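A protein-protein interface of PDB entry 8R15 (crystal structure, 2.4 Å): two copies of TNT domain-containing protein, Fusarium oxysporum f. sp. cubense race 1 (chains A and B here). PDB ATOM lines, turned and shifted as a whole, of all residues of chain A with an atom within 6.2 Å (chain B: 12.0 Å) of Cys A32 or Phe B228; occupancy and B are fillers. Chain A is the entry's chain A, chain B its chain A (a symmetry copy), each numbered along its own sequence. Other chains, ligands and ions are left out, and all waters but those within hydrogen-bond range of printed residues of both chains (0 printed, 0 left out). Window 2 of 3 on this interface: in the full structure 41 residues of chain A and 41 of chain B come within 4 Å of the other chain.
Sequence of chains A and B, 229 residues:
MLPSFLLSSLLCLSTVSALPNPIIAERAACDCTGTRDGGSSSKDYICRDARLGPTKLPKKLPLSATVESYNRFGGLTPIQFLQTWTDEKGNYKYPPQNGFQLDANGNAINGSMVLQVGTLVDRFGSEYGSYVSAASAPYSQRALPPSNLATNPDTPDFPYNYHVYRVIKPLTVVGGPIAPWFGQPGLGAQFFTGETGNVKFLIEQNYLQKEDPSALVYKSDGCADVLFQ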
ATOM      1  N   CYS A  30     -17.805  11.321   5.784  1.00  0.00           N
ATOM      2  CA  CYS A  30     -17.508  12.529   6.558  1.00  0.00           C
ATOM      3  C   CYS A  30     -16.420  13.350   5.882  1.00  0.00           C
ATOM      4  O   CYS A  30     -15.473  13.826   6.513  1.00  0.00           O
ATOM      5  CB  CYS A  30     -17.130  12.195   7.997  1.00  0.00           C
ATOM      6  SG  CYS A  30     -18.558  12.161   9.074  1.00  0.00           S
ATOM      7  N   ASP A  31     -16.572  13.520   4.578  1.00  0.00           N
ATOM      8  CA  ASP A  31     -15.580  14.179   3.754  1.00  0.00           C
ATOM      9  C   ASP A  31     -16.269  15.259   2.934  1.00  0.00           C
ATOM     10  O   ASP A  31     -17.498  15.382   2.928  1.00  0.00           O
ATOM     11  CB  ASP A  31     -14.864  13.162   2.854  1.00  0.00           C
ATOM     12  CG  ASP A  31     -13.457  13.583   2.498  1.00  0.00           C
ATOM     13  OD1 ASP A  31     -13.191  14.801   2.391  1.00  0.00           O
ATOM     14  OD2 ASP A  31     -12.610  12.686   2.316  1.00  0.00           O
ATOM     15  N   CYS A  32     -15.457  16.050   2.239  1.00  0.00           N
ATOM     16  CA  CYS A  32     -15.951  17.082   1.343  1.00  0.00           C
ATOM     17  C   CYS A  32     -16.201  16.554  -0.062  1.00  0.00           C
ATOM     18  O   CYS A  32     -16.289  17.348  -1.004  1.00  0.00           O
ATOM     19  CB  CYS A  32     -14.974  18.263   1.307  1.00  0.00           C
ATOM     20  SG  CYS A  32     -14.961  19.323   2.799  1.00  0.00           S
ATOM     21  N   THR A  33     -16.313  15.237  -0.219  1.00  0.00           N
ATOM     22  CA  THR A  33     -16.632  14.645  -1.511  1.00  0.00           C
ATOM     23  C   THR A  33     -18.034  15.053  -1.952  1.00  0.00           C
ATOM     24  O   THR A  33     -18.973  15.075  -1.150  1.00  0.00           O
ATOM     25  CB  THR A  33     -16.528  13.120  -1.426  1.00  0.00           C
ATOM     26  OG1 THR A  33     -15.186  12.754  -1.085  1.00  0.00           O
ATOM     27  CG2 THR A  33     -16.901  12.466  -2.740  1.00  0.00           C
ATOM     28  N   GLY A  34     -18.168  15.405  -3.231  1.00  0.00           N
ATOM     29  CA  GLY A  34     -19.445  15.788  -3.792  1.00  0.00           C
ATOM     30  C   GLY A  34     -19.837  17.233  -3.584  1.00  0.00           C
ATOM     31  O   GLY A  34     -20.824  17.685  -4.179  1.00  0.00           O
ATOM     32  N   THR A  35     -19.113  17.975  -2.758  1.00  0.00           N
ATOM     33  CA  THR A  35     -19.412  19.384  -2.591  1.00  0.00           C
ATOM     34  C   THR A  35     -18.819  20.179  -3.751  1.00  0.00           C
ATOM     35  O   THR A  35     -18.293  19.622  -4.720  1.00  0.00           O
ATOM     36  CB  THR A  35     -18.891  19.876  -1.246  1.00  0.00           C
ATOM     37  OG1 THR A  35     -17.468  19.722  -1.199  1.00  0.00           O
ATOM     38  CG2 THR A  35     -19.515  19.068  -0.131  1.00  0.00           C
ATOM     39  N   ARG A  36     -18.912  21.500  -3.655  1.00  0.00           N
ATOM     40  CA  ARG A  36     -18.472  22.406  -4.709  1.00  0.00           C
ATOM     41  C   ARG A  36     -17.497  23.408  -4.106  1.00  0.00           C
ATOM     42  O   ARG A  36     -17.907  24.322  -3.381  1.00  0.00           O
ATOM     43  CB  ARG A  36     -19.668  23.113  -5.343  1.00  0.00           C
ATOM     44  CG  ARG A  36     -19.333  23.969  -6.553  1.00  0.00           C
ATOM     45  CD  ARG A  36     -20.617  24.511  -7.154  1.00  0.00           C
ATOM     46  NE  ARG A  36     -21.548  23.429  -7.457  1.00  0.00           N
ATOM     47  CZ  ARG A  36     -22.868  23.531  -7.384  1.00  0.00           C
ATOM     48  NH1 ARG A  36     -23.454  24.649  -6.984  1.00  0.00           N
ATOM     49  NH2 ARG A  36     -23.618  22.481  -7.708  1.00  0.00           N
ATOM     50  N   ILE A  46     -18.283  25.703   5.006  1.00  0.00           N
ATOM     51  CA  ILE A  46     -17.937  24.290   5.114  1.00  0.00           C
ATOM     52  C   ILE A  46     -17.652  23.729   3.730  1.00  0.00           C
ATOM     53  O   ILE A  46     -18.465  23.858   2.805  1.00  0.00           O
ATOM     54  CB  ILE A  46     -19.070  23.515   5.805  1.00  0.00           C
ATOM     55  CG1 ILE A  46     -19.267  24.043   7.218  1.00  0.00           C
ATOM     56  CG2 ILE A  46     -18.755  22.035   5.851  1.00  0.00           C
ATOM     57  CD1 ILE A  46     -18.036  23.888   8.075  1.00  0.00           C
ATOM     58  N   CYS A  47     -16.482  23.112   3.580  1.00  0.00           N
ATOM     59  CA  CYS A  47     -16.020  22.563   2.310  1.00  0.00           C
ATOM     60  C   CYS A  47     -15.922  23.629   1.223  1.00  0.00           C
ATOM     61  O   CYS A  47     -15.902  23.308   0.031  1.00  0.00           O
ATOM     62  CB  CYS A  47     -16.917  21.411   1.853  1.00  0.00           C
ATOM     63  SG  CYS A  47     -16.865  20.003   2.982  1.00  0.00           S
ATOM     64  N   ARG A  48     -15.837  24.898   1.624  1.00  0.00           N
ATOM     65  CA  ARG A  48     -15.826  26.039   0.709  1.00  0.00           C
ATOM     66  C   ARG A  48     -17.041  26.027  -0.216  1.00  0.00           C
ATOM     67  O   ARG A  48     -16.985  26.526  -1.344  1.00  0.00           O
ATOM     68  CB  ARG A  48     -14.523  26.098  -0.093  1.00  0.00           C
ATOM     69  CG  ARG A  48     -13.288  25.768   0.740  1.00  0.00           C
ATOM     70  CD  ARG A  48     -12.149  26.739   0.495  1.00  0.00           C
ATOM     71  NE  ARG A  48     -11.483  26.511  -0.780  1.00  0.00           N
ATOM     72  CZ  ARG A  48     -10.525  25.615  -0.979  1.00  0.00           C
ATOM     73  NH1 ARG A  48     -10.114  24.814  -0.008  1.00  0.00           N
ATOM     74  NH2 ARG A  48      -9.969  25.516  -2.184  1.00  0.00           N
ATOM     75  N   PHE A  73     -26.154  18.817   8.442  1.00  0.00           N
ATOM     76  CA  PHE A  73     -26.378  17.812   7.413  1.00  0.00           C
ATOM     77  C   PHE A  73     -27.466  16.811   7.792  1.00  0.00           C
ATOM     78  O   PHE A  73     -27.694  15.847   7.050  1.00  0.00           O
ATOM     79  CB  PHE A  73     -25.066  17.084   7.102  1.00  0.00           C
ATOM     80  CG  PHE A  73     -23.952  18.000   6.641  1.00  0.00           C
ATOM     81  CD1 PHE A  73     -24.186  18.965   5.671  1.00  0.00           C
ATOM     82  CD2 PHE A  73     -22.680  17.906   7.187  1.00  0.00           C
ATOM     83  CE1 PHE A  73     -23.173  19.809   5.243  1.00  0.00           C
ATOM     84  CE2 PHE A  73     -21.660  18.746   6.768  1.00  0.00           C
ATOM     85  CZ  PHE A  73     -21.903  19.697   5.792  1.00  0.00           C
ATOM     86  N   THR A  77     -23.700  12.578   5.675  1.00  0.00           N
ATOM     87  CA  THR A  77     -22.475  13.138   5.136  1.00  0.00           C
ATOM     88  C   THR A  77     -22.828  14.133   4.026  1.00  0.00           C
ATOM     89  O   THR A  77     -23.918  14.049   3.446  1.00  0.00           O
ATOM     90  CB  THR A  77     -21.568  12.012   4.618  1.00  0.00           C
ATOM     91  OG1 THR A  77     -20.259  12.512   4.326  1.00  0.00           O
ATOM     92  CG2 THR A  77     -22.130  11.382   3.381  1.00  0.00           C
ATOM     93  N   PRO A  78     -21.956  15.124   3.761  1.00  0.00           N
ATOM     94  CA  PRO A  78     -22.298  16.151   2.756  1.00  0.00           C
ATOM     95  C   PRO A  78     -22.852  15.604   1.447  1.00  0.00           C
ATOM     96  O   PRO A  78     -23.898  16.082   0.987  1.00  0.00           O
ATOM     97  CB  PRO A  78     -20.963  16.892   2.568  1.00  0.00           C
ATOM     98  CG  PRO A  78     -20.322  16.823   3.915  1.00  0.00           C
ATOM     99  CD  PRO A  78     -20.756  15.499   4.533  1.00  0.00           C
ATOM    100  N   SER B 220     -24.641  13.229  19.644  1.00  0.00           N
ATOM    101  CA  SER B 220     -24.202  13.916  18.436  1.00  0.00           C
ATOM    102  C   SER B 220     -24.013  12.918  17.305  1.00  0.00           C
ATOM    103  O   SER B 220     -22.881  12.593  16.935  1.00  0.00           O
ATOM    104  CB  SER B 220     -22.908  14.691  18.698  1.00  0.00           C
ATOM    105  OG  SER B 220     -21.883  13.837  19.177  1.00  0.00           O
ATOM    106  N   ASP B 221     -25.118  12.422  16.753  1.00  0.00           N
ATOM    107  CA  ASP B 221     -25.079  11.418  15.692  1.00  0.00           C
ATOM    108  C   ASP B 221     -24.954  12.132  14.352  1.00  0.00           C
ATOM    109  O   ASP B 221     -25.945  12.600  13.785  1.00  0.00           O
ATOM    110  CB  ASP B 221     -26.320  10.533  15.743  1.00  0.00           C
ATOM    111  CG  ASP B 221     -27.592  11.327  15.966  1.00  0.00           C
ATOM    112  OD1 ASP B 221     -27.611  12.171  16.887  1.00  0.00           O
ATOM    113  OD2 ASP B 221     -28.566  11.114  15.213  1.00  0.00           O
ATOM    114  N   GLY B 222     -23.734  12.218  13.844  1.00  0.00           N
ATOM    115  CA  GLY B 222     -23.499  12.880  12.579  1.00  0.00           C
ATOM    116  C   GLY B 222     -22.043  13.278  12.451  1.00  0.00           C
ATOM    117  O   GLY B 222     -21.200  12.894  13.261  1.00  0.00           O
ATOM    118  N   CYS B 223     -21.772  14.055  11.402  1.00  0.00           N
ATOM    119  CA  CYS B 223     -20.437  14.579  11.135  1.00  0.00           C
ATOM    120  C   CYS B 223     -20.289  15.927  11.828  1.00  0.00           C
ATOM    121  O   CYS B 223     -21.000  16.881  11.495  1.00  0.00           O
ATOM    122  CB  CYS B 223     -20.195  14.732   9.635  1.00  0.00           C
ATOM    123  SG  CYS B 223     -20.252  13.210   8.681  1.00  0.00           S
ATOM    124  N   ALA B 224     -19.371  16.008  12.784  1.00  0.00           N
ATOM    125  CA  ALA B 224     -19.093  17.276  13.438  1.00  0.00           C
ATOM    126  C   ALA B 224     -18.351  18.215  12.489  1.00  0.00           C
ATOM    127  O   ALA B 224     -17.653  17.781  11.566  1.00  0.00           O
ATOM    128  CB  ALA B 224     -18.279  17.052  14.711  1.00  0.00           C
ATOM    129  N   ASP B 225     -18.518  19.521  12.719  1.00  0.00           N
ATOM    130  CA  ASP B 225     -17.877  20.512  11.861  1.00  0.00           C
ATOM    131  C   ASP B 225     -16.362  20.492  11.978  1.00  0.00           C
ATOM    132  O   ASP B 225     -15.677  20.974  11.071  1.00  0.00           O
ATOM    133  CB  ASP B 225     -18.398  21.913  12.183  1.00  0.00           C
ATOM    134  CG  ASP B 225     -19.883  22.060  11.909  1.00  0.00           C
ATOM    135  OD1 ASP B 225     -20.508  21.084  11.430  1.00  0.00           O
ATOM    136  OD2 ASP B 225     -20.422  23.155  12.175  1.00  0.00           O
ATOM    137  N   VAL B 226     -15.824  19.950  13.074  1.00  0.00           N
ATOM    138  CA  VAL B 226     -14.379  19.870  13.247  1.00  0.00           C
ATOM    139  C   VAL B 226     -13.725  18.968  12.213  1.00  0.00           C
ATOM    140  O   VAL B 226     -12.539  19.142  11.920  1.00  0.00           O
ATOM    141  CB  VAL B 226     -14.041  19.386  14.666  1.00  0.00           C
ATOM    142  CG1 VAL B 226     -14.670  20.310  15.722  1.00  0.00           C
ATOM    143  CG2 VAL B 226     -14.530  17.951  14.883  1.00  0.00           C
ATOM    144  N   LEU B 227     -14.473  18.034  11.623  1.00  0.00           N
ATOM    145  CA  LEU B 227     -13.925  17.146  10.606  1.00  0.00           C
ATOM    146  C   LEU B 227     -13.692  17.846   9.280  1.00  0.00           C
ATOM    147  O   LEU B 227     -13.315  17.175   8.314  1.00  0.00           O
ATOM    148  CB  LEU B 227     -14.857  15.951  10.403  1.00  0.00           C
ATOM    149  CG  LEU B 227     -15.382  15.279  11.676  1.00  0.00           C
ATOM    150  CD1 LEU B 227     -16.488  14.285  11.359  1.00  0.00           C
ATOM    151  CD2 LEU B 227     -14.255  14.606  12.443  1.00  0.00           C
ATOM    152  N   PHE B 228     -13.893  19.158   9.203  1.00  0.00           N
ATOM    153  CA  PHE B 228     -13.730  19.882   7.948  1.00  0.00           C
ATOM    154  C   PHE B 228     -12.820  21.100   8.105  1.00  0.00           C
ATOM    155  O   PHE B 228     -12.206  21.301   9.156  1.00  0.00           O
ATOM    156  CB  PHE B 228     -15.098  20.310   7.413  1.00  0.00           C
ATOM    157  CG  PHE B 228     -16.102  19.195   7.367  1.00  0.00           C
ATOM    158  CD1 PHE B 228     -16.142  18.324   6.291  1.00  0.00           C
ATOM    159  CD2 PHE B 228     -17.006  19.017   8.401  1.00  0.00           C
ATOM    160  CE1 PHE B 228     -17.065  17.296   6.244  1.00  0.00           C
ATOM    161  CE2 PHE B 228     -17.935  17.992   8.364  1.00  0.00           C
ATOM    162  CZ  PHE B 228     -17.965  17.129   7.285  1.00  0.00           C
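SG of Cys A30 forms a disulfide with SG of Cys B223.
N of Cys A30 sits at hydrogen-bond distance from OG1 of Thr A77 (3.1 Å). The backbone carbonyl oxygen of Cys A32 lies within hydrogen-bond range of the side-chain hydroxyl of Thr A35 (2.7 Å). The side-chain sulfur of Cys A32 is disulfide-bonded to the side-chain sulfur of Cys A47 (2.0 Å).
Cys A30 touches Leu B227. O of Cys A30 touches CE1 of Phe B228, at 3.8 Å. Asp A31 touches Phe B228. Phe B228 touches Cys A32 (CD1 to SG, 3.8 Å). Cys A47 touches Phe B228.
Cys A32 touches just one residue of chain B: Phe B228. Arg A36 touches none of the printed residues of chain B. No residue of chain B comes within 4 Å of Ile A46. Cys A47 touches just one residue of chain B: Phe B228 (3.8 Å). No residue of chain B comes within 4 Å of Pro A78. Of the printed residues of chain A, Cys B223 touches Cys A30 (2.0 Å). Asp B225 touches none of the printed residues of chain A. Of the printed residues of chain A, Leu B227 touches Cys A30 (3.7 Å). Phe B228 touches four residues of chain A. The nearest residue of chain B that does not touch Cys A32 is Leu B227 (6.1 Å).
Printed residues of chain A that touch a printed residue of chain B: Cys A30, Asp A31, Cys A32 and Cys A47. Of the 9 printed residues of chain B, 3 touch a printed residue of chain A. Hydrophobic or aromatic side chains of chain B within 4 Å of the printed part of chain A: Leu B227 and Phe B228. Along chain B the printed residues that touch a printed residue of chain A span positions 223 to 228. Among the printed residues, 6 pairs touch across the chains.
No position is printed for both chains.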
